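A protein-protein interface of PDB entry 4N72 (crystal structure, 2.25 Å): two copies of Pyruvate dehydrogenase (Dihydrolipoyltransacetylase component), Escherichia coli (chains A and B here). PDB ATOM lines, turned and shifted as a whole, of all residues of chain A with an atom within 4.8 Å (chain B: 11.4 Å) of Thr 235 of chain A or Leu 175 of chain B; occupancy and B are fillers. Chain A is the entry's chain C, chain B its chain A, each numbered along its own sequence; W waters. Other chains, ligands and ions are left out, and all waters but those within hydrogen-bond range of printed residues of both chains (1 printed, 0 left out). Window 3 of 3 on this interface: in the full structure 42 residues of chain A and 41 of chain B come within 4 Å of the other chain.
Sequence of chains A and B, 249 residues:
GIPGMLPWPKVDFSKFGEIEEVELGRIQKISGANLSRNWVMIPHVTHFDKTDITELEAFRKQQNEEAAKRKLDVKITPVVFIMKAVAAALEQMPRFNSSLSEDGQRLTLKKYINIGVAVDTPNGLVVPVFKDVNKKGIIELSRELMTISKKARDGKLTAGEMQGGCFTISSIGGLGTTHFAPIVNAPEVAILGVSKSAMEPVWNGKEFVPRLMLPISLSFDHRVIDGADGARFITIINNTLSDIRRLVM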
ATOM      1  N   ASP A  49     -28.218   2.215  27.615  1.00  0.00           N
ATOM      2  CA  ASP A  49     -28.769   2.984  26.506  1.00  0.00           C
ATOM      3  C   ASP A  49     -30.277   2.777  26.392  1.00  0.00           C
ATOM      4  O   ASP A  49     -30.845   1.903  27.049  1.00  0.00           O
ATOM      5  CB  ASP A  49     -28.079   2.590  25.196  1.00  0.00           C
ATOM      6  CG  ASP A  49     -28.283   3.611  24.093  1.00  0.00           C
ATOM      7  OD1 ASP A  49     -28.771   4.721  24.389  1.00  0.00           O
ATOM      8  OD2 ASP A  49     -27.945   3.303  22.930  1.00  0.00           O
ATOM      9  N   ALA A 228     -14.780   2.918  24.290  1.00  0.00           N
ATOM     10  CA  ALA A 228     -15.184   3.571  23.051  1.00  0.00           C
ATOM     11  C   ALA A 228     -15.840   2.579  22.096  1.00  0.00           C
ATOM     12  O   ALA A 228     -16.870   2.875  21.488  1.00  0.00           O
ATOM     13  CB  ALA A 228     -13.987   4.233  22.388  1.00  0.00           C
ATOM     14  N   ALA A 231     -19.262   1.636  23.215  1.00  0.00           N
ATOM     15  CA  ALA A 231     -20.235   2.681  22.922  1.00  0.00           C
ATOM     16  C   ALA A 231     -20.655   2.658  21.455  1.00  0.00           C
ATOM     17  O   ALA A 231     -21.803   2.957  21.129  1.00  0.00           O
ATOM     18  CB  ALA A 231     -19.678   4.047  23.297  1.00  0.00           C
ATOM     19  N   ARG A 232     -19.723   2.308  20.575  1.00  0.00           N
ATOM     20  CA  ARG A 232     -20.026   2.195  19.153  1.00  0.00           C
ATOM     21  C   ARG A 232     -20.948   1.011  18.895  1.00  0.00           C
ATOM     22  O   ARG A 232     -21.825   1.066  18.033  1.00  0.00           O
ATOM     23  CB  ARG A 232     -18.744   2.030  18.335  1.00  0.00           C
ATOM     24  CG  ARG A 232     -17.859   3.263  18.278  1.00  0.00           C
ATOM     25  CD  ARG A 232     -16.717   3.059  17.292  1.00  0.00           C
ATOM     26  NE  ARG A 232     -15.790   4.187  17.284  1.00  0.00           N
ATOM     27  CZ  ARG A 232     -14.682   4.246  18.016  1.00  0.00           C
ATOM     28  NH1 ARG A 232     -14.359   3.238  18.815  1.00  0.00           N
ATOM     29  NH2 ARG A 232     -13.896   5.310  17.947  1.00  0.00           N
ATOM     30  N   PHE A 233     -20.741  -0.061  19.653  1.00  0.00           N
ATOM     31  CA  PHE A 233     -21.498  -1.292  19.468  1.00  0.00           C
ATOM     32  C   PHE A 233     -22.950  -1.139  19.903  1.00  0.00           C
ATOM     33  O   PHE A 233     -23.870  -1.482  19.159  1.00  0.00           O
ATOM     34  CB  PHE A 233     -20.839  -2.437  20.238  1.00  0.00           C
ATOM     35  CG  PHE A 233     -21.367  -3.794  19.875  1.00  0.00           C
ATOM     36  CD1 PHE A 233     -20.992  -4.401  18.689  1.00  0.00           C
ATOM     37  CD2 PHE A 233     -22.232  -4.465  20.722  1.00  0.00           C
ATOM     38  CE1 PHE A 233     -21.473  -5.651  18.350  1.00  0.00           C
ATOM     39  CE2 PHE A 233     -22.717  -5.717  20.390  1.00  0.00           C
ATOM     40  CZ  PHE A 233     -22.338  -6.310  19.202  1.00  0.00           C
ATOM     41  N   ILE A 234     -23.153  -0.619  21.110  1.00  0.00           N
ATOM     42  CA  ILE A 234     -24.498  -0.434  21.644  1.00  0.00           C
ATOM     43  C   ILE A 234     -25.262   0.615  20.836  1.00  0.00           C
ATOM     44  O   ILE A 234     -26.490   0.584  20.771  1.00  0.00           O
ATOM     45  CB  ILE A 234     -24.471  -0.063  23.150  1.00  0.00           C
ATOM     46  CG1 ILE A 234     -25.830  -0.330  23.802  1.00  0.00           C
ATOM     47  CG2 ILE A 234     -24.026   1.382  23.354  1.00  0.00           C
ATOM     48  CD1 ILE A 234     -25.811  -0.199  25.311  1.00  0.00           C
ATOM     49  N   THR A 235     -24.527   1.528  20.205  1.00  0.00           N
ATOM     50  CA  THR A 235     -25.124   2.555  19.354  1.00  0.00           C
ATOM     51  C   THR A 235     -25.651   1.955  18.053  1.00  0.00           C
ATOM     52  O   THR A 235     -26.753   2.282  17.609  1.00  0.00           O
ATOM     53  CB  THR A 235     -24.112   3.676  19.032  1.00  0.00           C
ATOM     54  OG1 THR A 235     -23.864   4.450  20.212  1.00  0.00           O
ATOM     55  CG2 THR A 235     -24.644   4.591  17.936  1.00  0.00           C
ATOM     56  N   ILE A 236     -24.856   1.080  17.446  1.00  0.00           N
ATOM     57  CA  ILE A 236     -25.260   0.395  16.221  1.00  0.00           C
ATOM     58  C   ILE A 236     -26.530  -0.422  16.451  1.00  0.00           C
ATOM     59  O   ILE A 236     -27.452  -0.394  15.635  1.00  0.00           O
ATOM     60  CB  ILE A 236     -24.131  -0.508  15.683  1.00  0.00           C
ATOM     61  CG1 ILE A 236     -23.028   0.347  15.054  1.00  0.00           C
ATOM     62  CG2 ILE A 236     -24.669  -1.496  14.662  1.00  0.00           C
ATOM     63  CD1 ILE A 236     -21.778  -0.428  14.700  1.00  0.00           C
ATOM     64  N   ILE A 237     -26.574  -1.136  17.571  1.00  0.00           N
ATOM     65  CA  ILE A 237     -27.764  -1.877  17.974  1.00  0.00           C
ATOM     66  C   ILE A 237     -28.953  -0.932  18.126  1.00  0.00           C
ATOM     67  O   ILE A 237     -30.057  -1.227  17.667  1.00  0.00           O
ATOM     68  CB  ILE A 237     -27.530  -2.633  19.299  1.00  0.00           C
ATOM     69  CG1 ILE A 237     -26.537  -3.779  19.093  1.00  0.00           C
ATOM     70  CG2 ILE A 237     -28.841  -3.161  19.861  1.00  0.00           C
ATOM     71  CD1 ILE A 237     -26.263  -4.582  20.348  1.00  0.00           C
ATOM     72  N   ASN A 238     -28.709   0.208  18.766  1.00  0.00           N
ATOM     73  CA  ASN A 238     -29.719   1.248  18.932  1.00  0.00           C
ATOM     74  C   ASN A 238     -30.282   1.696  17.586  1.00  0.00           C
ATOM     75  O   ASN A 238     -31.489   1.623  17.355  1.00  0.00           O
ATOM     76  CB  ASN A 238     -29.116   2.444  19.678  1.00  0.00           C
ATOM     77  CG  ASN A 238     -30.161   3.443  20.150  1.00  0.00           C
ATOM     78  OD1 ASN A 238     -31.216   3.609  19.537  1.00  0.00           O
ATOM     79  ND2 ASN A 238     -29.862   4.125  21.249  1.00  0.00           N
ATOM     80  N   ASN A 239     -29.397   2.155  16.705  1.00  0.00           N
ATOM     81  CA  ASN A 239     -29.789   2.633  15.382  1.00  0.00           C
ATOM     82  C   ASN A 239     -30.516   1.573  14.561  1.00  0.00           C
ATOM     83  O   ASN A 239     -31.517   1.863  13.905  1.00  0.00           O
ATOM     84  CB  ASN A 239     -28.564   3.127  14.608  1.00  0.00           C
ATOM     85  CG  ASN A 239     -27.894   4.310  15.273  1.00  0.00           C
ATOM     86  OD1 ASN A 239     -28.555   5.145  15.891  1.00  0.00           O
ATOM     87  ND2 ASN A 239     -26.574   4.388  15.152  1.00  0.00           N
ATOM     88  N   ALA B 118      -9.337  10.446  29.103  1.00  0.00           N
ATOM     89  CA  ALA B 118      -9.326   9.443  28.042  1.00  0.00           C
ATOM     90  C   ALA B 118      -9.466  10.073  26.658  1.00  0.00           C
ATOM     91  O   ALA B 118     -10.386  10.853  26.409  1.00  0.00           O
ATOM     92  CB  ALA B 118     -10.422   8.414  28.272  1.00  0.00           C
ATOM     93  N   VAL B 119      -8.541   9.729  25.768  1.00  0.00           N
ATOM     94  CA  VAL B 119      -8.553  10.224  24.395  1.00  0.00           C
ATOM     95  C   VAL B 119      -8.473   9.044  23.430  1.00  0.00           C
ATOM     96  O   VAL B 119      -7.654   8.143  23.612  1.00  0.00           O
ATOM     97  CB  VAL B 119      -7.365  11.172  24.129  1.00  0.00           C
ATOM     98  CG1 VAL B 119      -7.419  11.710  22.708  1.00  0.00           C
ATOM     99  CG2 VAL B 119      -7.357  12.316  25.134  1.00  0.00           C
ATOM    100  N   ASP B 120      -9.320   9.047  22.404  1.00  0.00           N
ATOM    101  CA  ASP B 120      -9.351   7.938  21.453  1.00  0.00           C
ATOM    102  C   ASP B 120      -8.243   8.046  20.408  1.00  0.00           C
ATOM    103  O   ASP B 120      -7.943   9.131  19.913  1.00  0.00           O
ATOM    104  CB  ASP B 120     -10.719   7.834  20.776  1.00  0.00           C
ATOM    105  CG  ASP B 120     -10.934   6.489  20.107  1.00  0.00           C
ATOM    106  OD1 ASP B 120     -10.265   5.512  20.511  1.00  0.00           O
ATOM    107  OD2 ASP B 120     -11.771   6.404  19.184  1.00  0.00           O
ATOM    108  N   THR B 121      -7.639   6.906  20.089  1.00  0.00           N
ATOM    109  CA  THR B 121      -6.515   6.835  19.159  1.00  0.00           C
ATOM    110  C   THR B 121      -6.739   5.657  18.208  1.00  0.00           C
ATOM    111  O   THR B 121      -7.678   4.886  18.402  1.00  0.00           O
ATOM    112  CB  THR B 121      -5.185   6.634  19.924  1.00  0.00           C
ATOM    113  OG1 THR B 121      -5.180   5.349  20.556  1.00  0.00           O
ATOM    114  CG2 THR B 121      -4.991   7.719  20.973  1.00  0.00           C
ATOM    115  N   GLY B 124      -7.074   2.570  20.282  1.00  0.00           N
ATOM    116  CA  GLY B 124      -8.006   2.607  21.394  1.00  0.00           C
ATOM    117  C   GLY B 124      -7.813   3.806  22.303  1.00  0.00           C
ATOM    118  O   GLY B 124      -7.012   4.695  22.013  1.00  0.00           O
ATOM    119  N   LEU B 125      -8.553   3.827  23.407  1.00  0.00           N
ATOM    120  CA  LEU B 125      -8.467   4.917  24.373  1.00  0.00           C
ATOM    121  C   LEU B 125      -7.146   4.899  25.134  1.00  0.00           C
ATOM    122  O   LEU B 125      -6.697   3.849  25.591  1.00  0.00           O
ATOM    123  CB  LEU B 125      -9.627   4.842  25.371  1.00  0.00           C
ATOM    124  CG  LEU B 125     -11.032   5.194  24.882  1.00  0.00           C
ATOM    125  CD1 LEU B 125     -12.060   4.874  25.956  1.00  0.00           C
ATOM    126  CD2 LEU B 125     -11.115   6.660  24.484  1.00  0.00           C
ATOM    127  N   VAL B 126      -6.528   6.068  25.260  1.00  0.00           N
ATOM    128  CA  VAL B 126      -5.354   6.231  26.109  1.00  0.00           C
ATOM    129  C   VAL B 126      -5.623   7.357  27.100  1.00  0.00           C
ATOM    130  O   VAL B 126      -6.499   8.192  26.871  1.00  0.00           O
ATOM    131  CB  VAL B 126      -4.086   6.545  25.293  1.00  0.00           C
ATOM    132  CG1 VAL B 126      -3.776   5.405  24.333  1.00  0.00           C
ATOM    133  CG2 VAL B 126      -4.246   7.857  24.541  1.00  0.00           C
ATOM    134  N   SER B 170     -13.437   9.869  31.747  1.00  0.00           N
ATOM    135  CA  SER B 170     -13.657   9.176  30.482  1.00  0.00           C
ATOM    136  C   SER B 170     -14.975   9.617  29.852  1.00  0.00           C
ATOM    137  O   SER B 170     -16.049   9.206  30.289  1.00  0.00           O
ATOM    138  CB  SER B 170     -13.646   7.660  30.690  1.00  0.00           C
ATOM    139  OG  SER B 170     -13.701   6.974  29.451  1.00  0.00           O
ATOM    140  N   SER B 171     -14.883  10.457  28.826  1.00  0.00           N
ATOM    141  CA  SER B 171     -16.065  10.992  28.159  1.00  0.00           C
ATOM    142  C   SER B 171     -16.307  10.311  26.814  1.00  0.00           C
ATOM    143  O   SER B 171     -15.621  10.594  25.831  1.00  0.00           O
ATOM    144  CB  SER B 171     -15.928  12.503  27.965  1.00  0.00           C
ATOM    145  OG  SER B 171     -17.065  13.039  27.311  1.00  0.00           O
ATOM    146  N   ILE B 172     -17.293   9.420  26.776  1.00  0.00           N
ATOM    147  CA  ILE B 172     -17.586   8.651  25.571  1.00  0.00           C
ATOM    148  C   ILE B 172     -18.955   9.001  24.993  1.00  0.00           C
ATOM    149  O   ILE B 172     -19.457   8.314  24.102  1.00  0.00           O
ATOM    150  CB  ILE B 172     -17.531   7.136  25.851  1.00  0.00           C
ATOM    151  CG1 ILE B 172     -18.683   6.718  26.767  1.00  0.00           C
ATOM    152  CG2 ILE B 172     -16.193   6.758  26.469  1.00  0.00           C
ATOM    153  CD1 ILE B 172     -18.678   5.248  27.123  1.00  0.00           C
ATOM    154  N   GLY B 173     -19.548  10.077  25.501  1.00  0.00           N
ATOM    155  CA  GLY B 173     -20.873  10.498  25.080  1.00  0.00           C
ATOM    156  C   GLY B 173     -20.971  10.863  23.612  1.00  0.00           C
ATOM    157  O   GLY B 173     -22.053  10.819  23.025  1.00  0.00           O
ATOM    158  N   GLY B 174     -19.839  11.221  23.013  1.00  0.00           N
ATOM    159  CA  GLY B 174     -19.799  11.549  21.600  1.00  0.00           C
ATOM    160  C   GLY B 174     -20.024  10.328  20.728  1.00  0.00           C
ATOM    161  O   GLY B 174     -20.278  10.445  19.529  1.00  0.00           O
ATOM    162  N   LEU B 175     -19.931   9.151  21.338  1.00  0.00           N
ATOM    163  CA  LEU B 175     -20.138   7.894  20.632  1.00  0.00           C
ATOM    164  C   LEU B 175     -21.476   7.267  21.017  1.00  0.00           C
ATOM    165  O   LEU B 175     -22.110   6.593  20.207  1.00  0.00           O
ATOM    166  CB  LEU B 175     -18.998   6.923  20.940  1.00  0.00           C
ATOM    167  CG  LEU B 175     -17.587   7.436  20.651  1.00  0.00           C
ATOM    168  CD1 LEU B 175     -16.558   6.572  21.354  1.00  0.00           C
ATOM    169  CD2 LEU B 175     -17.324   7.469  19.155  1.00  0.00           C
ATOM    170  N   GLY B 176     -21.897   7.489  22.259  1.00  0.00           N
ATOM    171  CA  GLY B 176     -23.176   6.980  22.722  1.00  0.00           C
ATOM    172  C   GLY B 176     -23.260   6.674  24.207  1.00  0.00           C
ATOM    173  O   GLY B 176     -22.472   7.188  25.004  1.00  0.00           O
ATOM    174  N   THR B 177     -24.222   5.816  24.553  1.00  0.00           N
ATOM    175  CA  THR B 177     -24.586   5.448  25.931  1.00  0.00           C
ATOM    176  C   THR B 177     -25.310   6.559  26.689  1.00  0.00           C
ATOM    177  O   THR B 177     -25.067   7.742  26.463  1.00  0.00           O
ATOM    178  CB  THR B 177     -23.394   4.942  26.789  1.00  0.00           C
ATOM    179  OG1 THR B 177     -22.616   6.057  27.242  1.00  0.00           O
ATOM    180  CG2 THR B 177     -22.519   3.970  26.003  1.00  0.00           C
ATOM    181  N   THR B 178     -26.202   6.161  27.591  1.00  0.00           N
ATOM    182  CA  THR B 178     -26.917   7.100  28.446  1.00  0.00           C
ATOM    183  C   THR B 178     -26.302   7.111  29.840  1.00  0.00           C
ATOM    184  O   THR B 178     -26.579   7.999  30.644  1.00  0.00           O
ATOM    185  CB  THR B 178     -28.407   6.730  28.560  1.00  0.00           C
ATOM    186  OG1 THR B 178     -28.530   5.348  28.912  1.00  0.00           O
ATOM    187  CG2 THR B 178     -29.121   6.973  27.240  1.00  0.00           C
ATOM    188  N   HIS B 179     -25.465   6.112  30.105  1.00  0.00           N
ATOM    189  CA  HIS B 179     -24.774   5.938  31.379  1.00  0.00           C
ATOM    190  C   HIS B 179     -23.857   4.735  31.231  1.00  0.00           C
ATOM    191  O   HIS B 179     -24.145   3.833  30.447  1.00  0.00           O
ATOM    192  CB  HIS B 179     -25.769   5.667  32.512  1.00  0.00           C
ATOM    193  CG  HIS B 179     -26.108   6.876  33.333  1.00  0.00           C
ATOM    194  ND1 HIS B 179     -27.405   7.264  33.581  1.00  0.00           N
ATOM    195  CD2 HIS B 179     -25.315   7.770  33.969  1.00  0.00           C
ATOM    196  CE1 HIS B 179     -27.400   8.351  34.332  1.00  0.00           C
ATOM    197  NE2 HIS B 179     -26.148   8.681  34.582  1.00  0.00           N
ATOM    198  N   PHE B 180     -22.752   4.714  31.971  1.00  0.00           N
ATOM    199  CA  PHE B 180     -21.914   3.517  32.010  1.00  0.00           C
ATOM    200  C   PHE B 180     -21.124   3.374  33.309  1.00  0.00           C
ATOM    201  O   PHE B 180     -20.932   4.343  34.041  1.00  0.00           O
ATOM    202  CB  PHE B 180     -21.008   3.412  30.772  1.00  0.00           C
ATOM    203  CG  PHE B 180     -19.876   4.404  30.740  1.00  0.00           C
ATOM    204  CD1 PHE B 180     -20.114   5.746  30.492  1.00  0.00           C
ATOM    205  CD2 PHE B 180     -18.567   3.983  30.916  1.00  0.00           C
ATOM    206  CE1 PHE B 180     -19.069   6.654  30.447  1.00  0.00           C
ATOM    207  CE2 PHE B 180     -17.520   4.886  30.871  1.00  0.00           C
ATOM    208  CZ  PHE B 180     -17.772   6.221  30.637  1.00  0.00           C
ATOM    209  N   VAL B 194     -18.599  10.062  31.482  1.00  0.00           N
ATOM    210  CA  VAL B 194     -19.535  11.022  30.905  1.00  0.00           C
ATOM    211  C   VAL B 194     -20.220  10.433  29.674  1.00  0.00           C
ATOM    212  O   VAL B 194     -19.554   9.981  28.743  1.00  0.00           O
ATOM    213  CB  VAL B 194     -18.832  12.337  30.512  1.00  0.00           C
ATOM    214  CG1 VAL B 194     -19.853  13.369  30.058  1.00  0.00           C
ATOM    215  CG2 VAL B 194     -18.015  12.875  31.676  1.00  0.00           C
ATOM    216  N   SER B 195     -21.549  10.440  29.673  1.00  0.00           N
ATOM    217  CA  SER B 195     -22.316   9.889  28.558  1.00  0.00           C
ATOM    218  C   SER B 195     -22.990  10.983  27.730  1.00  0.00           C
ATOM    219  O   SER B 195     -22.732  12.170  27.930  1.00  0.00           O
ATOM    220  CB  SER B 195     -23.350   8.878  29.059  1.00  0.00           C
ATOM    221  OG  SER B 195     -22.716   7.738  29.614  1.00  0.00           O
ATOM    222  N   LYS B 196     -23.852  10.577  26.800  1.00  0.00           N
ATOM    223  CA  LYS B 196     -24.458  11.515  25.857  1.00  0.00           C
ATOM    224  C   LYS B 196     -25.534  12.384  26.506  1.00  0.00           C
ATOM    225  O   LYS B 196     -26.387  11.895  27.249  1.00  0.00           O
ATOM    226  CB  LYS B 196     -25.020  10.780  24.631  1.00  0.00           C
ATOM    227  CG  LYS B 196     -26.350  10.073  24.859  1.00  0.00           C
ATOM    228  CD  LYS B 196     -26.736   9.193  23.682  1.00  0.00           C
ATOM    229  CE  LYS B 196     -28.016   8.427  23.978  1.00  0.00           C
ATOM    230  NZ  LYS B 196     -28.399   7.520  22.860  1.00  0.00           N
ATOM    231  N   SER B 197     -25.483  13.681  26.224  1.00  0.00           N
ATOM    232  CA  SER B 197     -26.466  14.615  26.755  1.00  0.00           C
ATOM    233  C   SER B 197     -27.753  14.562  25.938  1.00  0.00           C
ATOM    234  O   SER B 197     -27.748  14.141  24.780  1.00  0.00           O
ATOM    235  CB  SER B 197     -25.906  16.038  26.764  1.00  0.00           C
ATOM    236  OG  SER B 197     -25.647  16.491  25.445  1.00  0.00           O
ATOM    237  N   LEU B 214     -26.898  16.313  31.191  1.00  0.00           N
ATOM    238  CA  LEU B 214     -25.704  15.515  30.953  1.00  0.00           C
ATOM    239  C   LEU B 214     -25.571  14.423  32.007  1.00  0.00           C
ATOM    240  O   LEU B 214     -25.375  14.717  33.186  1.00  0.00           O
ATOM    241  CB  LEU B 214     -24.457  16.399  30.974  1.00  0.00           C
ATOM    242  CG  LEU B 214     -23.125  15.682  30.737  1.00  0.00           C
ATOM    243  CD1 LEU B 214     -22.950  15.330  29.263  1.00  0.00           C
ATOM    244  CD2 LEU B 214     -21.959  16.518  31.244  1.00  0.00           C
ATOM    245  N   PRO B 215     -25.660  13.169  31.578  1.00  0.00           N
ATOM    246  CA  PRO B 215     -25.525  12.031  32.494  1.00  0.00           C
ATOM    247  C   PRO B 215     -24.063  11.729  32.817  1.00  0.00           C
ATOM    248  O   PRO B 215     -23.238  11.634  31.908  1.00  0.00           O
ATOM    249  CB  PRO B 215     -26.138  10.876  31.702  1.00  0.00           C
ATOM    250  CG  PRO B 215     -25.929  11.250  30.278  1.00  0.00           C
ATOM    251  CD  PRO B 215     -26.058  12.746  30.223  1.00  0.00           C
HETATM  252  O   HOH W   1     -25.793   5.118  22.284  1.00  0.00           O
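No position is printed for both chains.
Of the 24 printed residues of chain B, 7 touch a printed residue of chain A.
Printed residues of chain A that touch a printed residue of chain B: Asp 49, Ala 228, Ala 231, Arg 232, Ile 234 and Thr 235.
Hydrophobic or aromatic side chains of chain A that line the printed part of chain B: Ala 228, Ala 231 and Ile 234.
Among the printed residues, Asp or Glu carboxylates within 4 Å of a Lys or Arg side-chain nitrogen of the other chain: Asp 49 of chain A with Lys 196 of chain B and Arg 232 of chain A with Asp 120 of chain B.
Thr 235 of chain A touches just these residues of chain B: Leu 175 (2.8 Å) and Gly 176 (3.6 Å).
Printed residues of chain A within 4 Å of Leu 175 of chain B: Ala 228 (3.6 Å), Ala 231 (3.8 Å) and Thr 235 (2.8 Å).
Ala 231 of chain A touches two residues of chain B.
Arg 232 of chain A touches one residue of chain B.
No residue of chain B comes within 4 Å of Ile 236 of chain A.
No residue of chain B comes within 4 Å of Ile 237 of chain A.
Asn 238 of chain A touches none of the printed residues of chain B.
Asn 239 of chain A touches none of the printed residues of chain B.
Of the printed residues of chain B, Ile 234 of chain A touches Thr 177 (3.998 Å).
Of the printed residues of chain A, Asp 120 of chain B touches Arg 232 (2.7 Å).
Printed residues of chain A within 4 Å of Gly 176 of chain B: Thr 235 (3.6 Å).
Printed residues of chain A within 4 Å of Leu 125 of chain B: Ala 228.
Printed residues of chain A within 4 Å of Thr 177 of chain B: Ala 231 and Ile 234.
Ser 171 of chain B touches none of the printed residues of chain A.
Ile 172 of chain B touches none of the printed residues of chain A.
OD2 of Asp 120 of chain B is in salt-bridge range of NH2 of Arg 232 of chain A (2.7 Å).
OG1 of Thr 235 of chain A lies within hydrogen-bond range of O of Leu 175 of chain B, 2.8 Å away.
The backbone NH (N) of Asp 49 of chain A sits close to the side-chain hydroxyl (OG1) of Thr 178 of chain B (3.4 Å).
NZ of Lys 196 of chain B lies within salt-bridge range of OD1 of Asp 49 of chain A, 3.2 Å away.
The side-chain amide nitrogen (ND2) of Asn 239 of chain A is in hydrogen-bond range of the backbone carbonyl oxygen (O) of Thr 235 of chain A.
OG1 of Thr 177 of chain B is in hydrogen-bond range of OG of Ser 195 of chain B, 2.9 Å away.
The backbone carbonyl oxygen (O) of Thr 177 of chain B is in hydrogen-bond range of the backbone NH (N) of Lys 196 of chain B (3.1 Å).
OD2 of Asp 49 of chain A sits at hydrogen-bond distance from ND2 of Asn 238 of chain A (2.7 Å).
O of Ala 231 of chain A is in hydrogen-bond range of OG1 of Thr 235 of chain A (2.7 Å).
Water W1 lies within hydrogen-bond range of N of Thr 177 of chain B, OD2 of Asp 49 of chain A and OG1 of Thr 235 of chain A.
Leu 125 of chain B touches Ala 228 of chain A.
CD1 of Leu 175 of chain B touches CB of Ala 228 of chain A, 3.6 Å away.
Leu 175 of chain B touches Ala 231 of chain A (O to O, 3.8 Å).
CB of Ala 231 of chain A touches CG2 of Thr 177 of chain B, 3.9 Å away.
Thr 177 of chain B touches Ile 234 of chain A (CG2 to CG2, 3.998 Å).
OG1 of Thr 235 of chain A touches CA of Gly 176 of chain B, 3.6 Å away.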
